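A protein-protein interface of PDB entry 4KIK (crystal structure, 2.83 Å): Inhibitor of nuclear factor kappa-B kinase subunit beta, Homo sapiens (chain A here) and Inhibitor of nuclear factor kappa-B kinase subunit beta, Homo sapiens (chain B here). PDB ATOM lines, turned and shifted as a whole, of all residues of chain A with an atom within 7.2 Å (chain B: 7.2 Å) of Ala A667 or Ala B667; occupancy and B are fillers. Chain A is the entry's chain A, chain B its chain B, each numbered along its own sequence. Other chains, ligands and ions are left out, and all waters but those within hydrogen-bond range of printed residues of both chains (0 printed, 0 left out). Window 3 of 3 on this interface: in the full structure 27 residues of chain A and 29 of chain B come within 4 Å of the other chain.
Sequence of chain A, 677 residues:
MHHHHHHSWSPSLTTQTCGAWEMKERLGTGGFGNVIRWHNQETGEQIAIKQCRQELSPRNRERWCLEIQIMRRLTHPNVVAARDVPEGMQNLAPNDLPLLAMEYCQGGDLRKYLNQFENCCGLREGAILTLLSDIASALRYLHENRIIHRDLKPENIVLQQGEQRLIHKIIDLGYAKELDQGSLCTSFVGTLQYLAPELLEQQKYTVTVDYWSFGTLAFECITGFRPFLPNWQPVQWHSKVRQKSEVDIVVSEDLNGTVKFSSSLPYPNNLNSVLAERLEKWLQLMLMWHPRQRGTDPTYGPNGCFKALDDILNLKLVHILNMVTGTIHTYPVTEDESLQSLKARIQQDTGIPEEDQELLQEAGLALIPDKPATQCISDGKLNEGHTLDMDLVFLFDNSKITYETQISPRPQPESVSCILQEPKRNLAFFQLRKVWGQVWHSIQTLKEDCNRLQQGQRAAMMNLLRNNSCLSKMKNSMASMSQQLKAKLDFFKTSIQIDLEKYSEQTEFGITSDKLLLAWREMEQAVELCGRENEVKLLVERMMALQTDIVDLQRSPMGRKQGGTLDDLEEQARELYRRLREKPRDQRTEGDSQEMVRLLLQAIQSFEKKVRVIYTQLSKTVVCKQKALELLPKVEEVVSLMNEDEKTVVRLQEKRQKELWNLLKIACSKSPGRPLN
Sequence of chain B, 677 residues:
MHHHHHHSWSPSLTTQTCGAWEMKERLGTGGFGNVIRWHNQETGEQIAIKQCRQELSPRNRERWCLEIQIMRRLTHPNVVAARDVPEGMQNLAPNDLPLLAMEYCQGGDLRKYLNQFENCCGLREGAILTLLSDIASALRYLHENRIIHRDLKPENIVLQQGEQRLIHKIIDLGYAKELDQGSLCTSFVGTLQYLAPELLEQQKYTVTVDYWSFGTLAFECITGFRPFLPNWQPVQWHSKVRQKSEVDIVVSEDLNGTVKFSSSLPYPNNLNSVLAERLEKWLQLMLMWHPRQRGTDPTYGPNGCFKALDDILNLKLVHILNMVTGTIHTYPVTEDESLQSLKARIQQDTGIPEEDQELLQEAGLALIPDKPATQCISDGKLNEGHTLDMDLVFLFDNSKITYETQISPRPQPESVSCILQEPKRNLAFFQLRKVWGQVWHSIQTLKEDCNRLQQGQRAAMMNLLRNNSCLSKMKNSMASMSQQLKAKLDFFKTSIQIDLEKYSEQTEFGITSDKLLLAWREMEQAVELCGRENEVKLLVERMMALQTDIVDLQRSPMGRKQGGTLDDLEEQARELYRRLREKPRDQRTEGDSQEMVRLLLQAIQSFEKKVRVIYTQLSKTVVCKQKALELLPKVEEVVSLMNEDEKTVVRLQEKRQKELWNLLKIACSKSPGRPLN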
ATOM      1  N   GLN A 506      18.899 -14.728   8.307  1.00  0.00           N
ATOM      2  CA  GLN A 506      18.916 -14.986   9.756  1.00  0.00           C
ATOM      3  C   GLN A 506      18.876 -13.603  10.514  1.00  0.00           C
ATOM      4  O   GLN A 506      19.905 -13.032  10.896  1.00  0.00           O
ATOM      5  CB  GLN A 506      20.138 -15.890  10.098  1.00  0.00           C
ATOM      6  CG  GLN A 506      20.611 -15.997  11.554  1.00  0.00           C
ATOM      7  CD  GLN A 506      21.595 -14.915  11.993  1.00  0.00           C
ATOM      8  OE1 GLN A 506      21.665 -14.571  13.171  1.00  0.00           O
ATOM      9  NE2 GLN A 506      22.364 -14.319  11.089  1.00  0.00           N
ATOM     10  N   ASN A 662      32.974 -16.309  14.568  1.00  0.00           N
ATOM     11  CA  ASN A 662      32.831 -15.353  15.653  1.00  0.00           C
ATOM     12  C   ASN A 662      31.361 -15.182  15.992  1.00  0.00           C
ATOM     13  O   ASN A 662      31.029 -15.029  17.164  1.00  0.00           O
ATOM     14  CB  ASN A 662      33.456 -14.023  15.256  1.00  0.00           C
ATOM     15  CG  ASN A 662      34.311 -13.380  16.307  1.00  0.00           C
ATOM     16  OD1 ASN A 662      34.422 -13.841  17.444  1.00  0.00           O
ATOM     17  ND2 ASN A 662      34.955 -12.302  15.932  1.00  0.00           N
ATOM     18  N   LEU A 663      30.482 -15.225  14.983  1.00  0.00           N
ATOM     19  CA  LEU A 663      29.036 -15.134  15.189  1.00  0.00           C
ATOM     20  C   LEU A 663      28.556 -16.336  15.987  1.00  0.00           C
ATOM     21  O   LEU A 663      27.761 -16.190  16.936  1.00  0.00           O
ATOM     22  CB  LEU A 663      28.285 -15.070  13.849  1.00  0.00           C
ATOM     23  CG  LEU A 663      28.061 -13.685  13.243  1.00  0.00           C
ATOM     24  CD1 LEU A 663      28.271 -13.741  11.755  1.00  0.00           C
ATOM     25  CD2 LEU A 663      26.701 -13.106  13.585  1.00  0.00           C
ATOM     26  N   LEU A 664      29.092 -17.528  15.615  1.00  0.00           N
ATOM     27  CA  LEU A 664      28.804 -18.815  16.243  1.00  0.00           C
ATOM     28  C   LEU A 664      29.292 -18.853  17.692  1.00  0.00           C
ATOM     29  O   LEU A 664      28.752 -19.619  18.479  1.00  0.00           O
ATOM     30  CB  LEU A 664      29.441 -19.956  15.430  1.00  0.00           C
ATOM     31  CG  LEU A 664      28.828 -21.344  15.613  1.00  0.00           C
ATOM     32  CD1 LEU A 664      27.569 -21.491  14.807  1.00  0.00           C
ATOM     33  CD2 LEU A 664      29.797 -22.421  15.224  1.00  0.00           C
ATOM     34  N   LYS A 665      30.296 -18.029  18.053  1.00  0.00           N
ATOM     35  CA  LYS A 665      30.801 -17.946  19.426  1.00  0.00           C
ATOM     36  C   LYS A 665      29.735 -17.271  20.267  1.00  0.00           C
ATOM     37  O   LYS A 665      29.216 -17.881  21.210  1.00  0.00           O
ATOM     38  CB  LYS A 665      32.135 -17.172  19.491  1.00  0.00           C
ATOM     39  CG  LYS A 665      33.112 -17.741  20.495  1.00  0.00           C
ATOM     40  CD  LYS A 665      34.247 -16.788  20.793  1.00  0.00           C
ATOM     41  CE  LYS A 665      35.139 -17.349  21.868  1.00  0.00           C
ATOM     42  NZ  LYS A 665      36.159 -16.366  22.322  1.00  0.00           N
ATOM     43  N   ILE A 666      29.352 -16.032  19.856  1.00  0.00           N
ATOM     44  CA  ILE A 666      28.358 -15.156  20.496  1.00  0.00           C
ATOM     45  C   ILE A 666      27.029 -15.927  20.694  1.00  0.00           C
ATOM     46  O   ILE A 666      26.474 -15.901  21.795  1.00  0.00           O
ATOM     47  CB  ILE A 666      28.195 -13.841  19.677  1.00  0.00           C
ATOM     48  CG1 ILE A 666      29.549 -13.105  19.565  1.00  0.00           C
ATOM     49  CG2 ILE A 666      27.152 -12.936  20.299  1.00  0.00           C
ATOM     50  CD1 ILE A 666      29.725 -12.126  18.464  1.00  0.00           C
ATOM     51  N   ALA A 667      26.578 -16.661  19.660  1.00  0.00           N
ATOM     52  CA  ALA A 667      25.357 -17.459  19.709  1.00  0.00           C
ATOM     53  C   ALA A 667      25.494 -18.661  20.658  1.00  0.00           C
ATOM     54  O   ALA A 667      24.492 -19.050  21.273  1.00  0.00           O
ATOM     55  CB  ALA A 667      24.989 -17.931  18.317  1.00  0.00           C
ATOM     56  N   CYS A 668      26.730 -19.208  20.828  1.00  0.00           N
ATOM     57  CA  CYS A 668      27.002 -20.360  21.712  1.00  0.00           C
ATOM     58  C   CYS A 668      27.082 -19.965  23.207  1.00  0.00           C
ATOM     59  O   CYS A 668      27.446 -20.822  24.022  1.00  0.00           O
ATOM     60  CB  CYS A 668      28.267 -21.099  21.280  1.00  0.00           C
ATOM     61  SG  CYS A 668      27.977 -22.461  20.119  1.00  0.00           S
ATOM     62  N   SER A 669      26.742 -18.696  23.570  1.00  0.00           N
ATOM     63  CA  SER A 669      26.774 -18.208  24.957  1.00  0.00           C
ATOM     64  C   SER A 669      25.414 -17.645  25.410  1.00  0.00           C
ATOM     65  O   SER A 669      24.675 -17.051  24.621  1.00  0.00           O
ATOM     66  CB  SER A 669      27.862 -17.157  25.129  1.00  0.00           C
ATOM     67  OG  SER A 669      27.597 -16.016  24.334  1.00  0.00           O
ATOM     68  N   ILE B 511      29.893 -26.031  19.835  1.00  0.00           N
ATOM     69  CA  ILE B 511      29.160 -27.131  19.198  1.00  0.00           C
ATOM     70  C   ILE B 511      30.108 -28.230  18.737  1.00  0.00           C
ATOM     71  O   ILE B 511      31.120 -27.941  18.100  1.00  0.00           O
ATOM     72  CB  ILE B 511      28.292 -26.609  18.022  1.00  0.00           C
ATOM     73  CG1 ILE B 511      27.100 -25.748  18.508  1.00  0.00           C
ATOM     74  CG2 ILE B 511      27.830 -27.740  17.097  1.00  0.00           C
ATOM     75  CD1 ILE B 511      25.951 -26.504  19.355  1.00  0.00           C
ATOM     76  N   ASN B 662      24.012 -23.122   8.940  1.00  0.00           N
ATOM     77  CA  ASN B 662      23.075 -24.054   9.542  1.00  0.00           C
ATOM     78  C   ASN B 662      23.394 -24.224  11.018  1.00  0.00           C
ATOM     79  O   ASN B 662      22.471 -24.381  11.815  1.00  0.00           O
ATOM     80  CB  ASN B 662      23.158 -25.399   8.829  1.00  0.00           C
ATOM     81  CG  ASN B 662      21.829 -26.047   8.520  1.00  0.00           C
ATOM     82  OD1 ASN B 662      20.747 -25.577   8.917  1.00  0.00           O
ATOM     83  ND2 ASN B 662      21.892 -27.148   7.770  1.00  0.00           N
ATOM     84  N   LEU B 663      24.688 -24.195  11.389  1.00  0.00           N
ATOM     85  CA  LEU B 663      25.118 -24.298  12.783  1.00  0.00           C
ATOM     86  C   LEU B 663      24.627 -23.084  13.551  1.00  0.00           C
ATOM     87  O   LEU B 663      24.117 -23.223  14.666  1.00  0.00           O
ATOM     88  CB  LEU B 663      26.642 -24.398  12.877  1.00  0.00           C
ATOM     89  CG  LEU B 663      27.285 -25.759  13.023  1.00  0.00           C
ATOM     90  CD1 LEU B 663      26.559 -26.834  12.252  1.00  0.00           C
ATOM     91  CD2 LEU B 663      28.753 -25.688  12.688  1.00  0.00           C
ATOM     92  N   LEU B 664      24.727 -21.898  12.905  1.00  0.00           N
ATOM     93  CA  LEU B 664      24.302 -20.613  13.446  1.00  0.00           C
ATOM     94  C   LEU B 664      22.777 -20.557  13.634  1.00  0.00           C
ATOM     95  O   LEU B 664      22.302 -19.804  14.472  1.00  0.00           O
ATOM     96  CB  LEU B 664      24.801 -19.476  12.539  1.00  0.00           C
ATOM     97  CG  LEU B 664      24.779 -18.064  13.146  1.00  0.00           C
ATOM     98  CD1 LEU B 664      25.868 -17.874  14.166  1.00  0.00           C
ATOM     99  CD2 LEU B 664      24.855 -17.016  12.096  1.00  0.00           C
ATOM    100  N   LYS B 665      22.018 -21.367  12.892  1.00  0.00           N
ATOM    101  CA  LYS B 665      20.562 -21.452  13.055  1.00  0.00           C
ATOM    102  C   LYS B 665      20.267 -22.160  14.366  1.00  0.00           C
ATOM    103  O   LYS B 665      19.639 -21.574  15.252  1.00  0.00           O
ATOM    104  CB  LYS B 665      19.912 -22.199  11.872  1.00  0.00           C
ATOM    105  CG  LYS B 665      18.629 -21.562  11.369  1.00  0.00           C
ATOM    106  CD  LYS B 665      18.937 -20.421  10.390  1.00  0.00           C
ATOM    107  CE  LYS B 665      17.715 -19.731   9.828  1.00  0.00           C
ATOM    108  NZ  LYS B 665      18.089 -18.558   8.987  1.00  0.00           N
ATOM    109  N   ILE B 666      20.813 -23.392  14.512  1.00  0.00           N
ATOM    110  CA  ILE B 666      20.690 -24.275  15.677  1.00  0.00           C
ATOM    111  C   ILE B 666      21.105 -23.528  16.963  1.00  0.00           C
ATOM    112  O   ILE B 666      20.380 -23.591  17.957  1.00  0.00           O
ATOM    113  CB  ILE B 666      21.506 -25.584  15.452  1.00  0.00           C
ATOM    114  CG1 ILE B 666      20.981 -26.329  14.201  1.00  0.00           C
ATOM    115  CG2 ILE B 666      21.477 -26.500  16.690  1.00  0.00           C
ATOM    116  CD1 ILE B 666      21.952 -27.313  13.561  1.00  0.00           C
ATOM    117  N   ALA B 667      22.221 -22.788  16.919  1.00  0.00           N
ATOM    118  CA  ALA B 667      22.715 -22.005  18.054  1.00  0.00           C
ATOM    119  C   ALA B 667      21.799 -20.806  18.370  1.00  0.00           C
ATOM    120  O   ALA B 667      21.720 -20.404  19.533  1.00  0.00           O
ATOM    121  CB  ALA B 667      24.129 -21.522  17.787  1.00  0.00           C
ATOM    122  N   CYS B 668      21.081 -20.267  17.357  1.00  0.00           N
ATOM    123  CA  CYS B 668      20.169 -19.130  17.536  1.00  0.00           C
ATOM    124  C   CYS B 668      18.785 -19.562  18.104  1.00  0.00           C
ATOM    125  O   CYS B 668      17.883 -18.724  18.163  1.00  0.00           O
ATOM    126  CB  CYS B 668      20.011 -18.349  16.232  1.00  0.00           C
ATOM    127  SG  CYS B 668      21.205 -16.994  16.018  1.00  0.00           S
ATOM    128  N   SER B 669      18.628 -20.840  18.549  1.00  0.00           N
ATOM    129  CA  SER B 669      17.372 -21.376  19.113  1.00  0.00           C
ATOM    130  C   SER B 669      17.572 -22.003  20.510  1.00  0.00           C
ATOM    131  O   SER B 669      18.603 -22.613  20.804  1.00  0.00           O
ATOM    132  CB  SER B 669      16.748 -22.400  18.170  1.00  0.00           C
ATOM    133  OG  SER B 669      17.580 -23.536  17.995  1.00  0.00           O
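Of the 9 printed residues of chain B, 6 touch a printed residue of chain A.
Hydrophobic or aromatic side chains of chain B that line the printed part of chain A: Ile B511, Leu B663, Leu B664 and Ala B667.
Of the 9 printed residues of chain A, 5 touch a printed residue of chain B.
Hydrophobic or aromatic side chains of chain A within 4 Å of the printed part of chain B: Leu A663, Leu A664 and Ala A667.
Among the printed residues, 8 pairs touch across the chains.
Among the printed residues, no Asp or Glu carboxylate lies within 4 Å of a Lys or Arg side-chain nitrogen of the other chain.
Of the printed residues of chain B, Leu A664 touches Leu B663 (3.6 Å) and Leu B664 (3.4 Å).
Printed residues of chain B within 4 Å of Ala A667: Ala B667 (3.5 Å).
Ala B667 touches just one residue of chain A: Ala A667 (3.5 Å).
Printed residues of chain A within 4 Å of Cys B668: Gln A506 (3.8 Å).
The nearest residue of chain A that does not touch Ala B667 is Leu A664 (4.6 Å).
The nearest printed residue of chain A that does not touch Leu B664 is Ala A667 (4.2 Å).
Among the printed residues, pairs that only touch across the chains: Leu A664 with Leu B664 (3.4 Å), Ala A667 with Ala B667 (3.5 Å), Gln A506 with Lys B665 (3.5 Å), Leu A664 with Leu B663 (3.6 Å), Leu A663 with Leu B664 (3.6 Å), Cys A668 with Ile B511 (3.8 Å) and Gln A506 with Leu B664 (3.8 Å).
The side-chain amide oxygen of Gln A506 lies within hydrogen-bond range of the side-chain sulfur of Cys B668 (3.8 Å).
The side-chain sulfur (SG) of Cys A668 lies close to the backbone carbonyl oxygen (O) of Leu A664 (3.4 Å).
SG of Cys B668 lies close to O of Leu B664 (3.4 Å).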
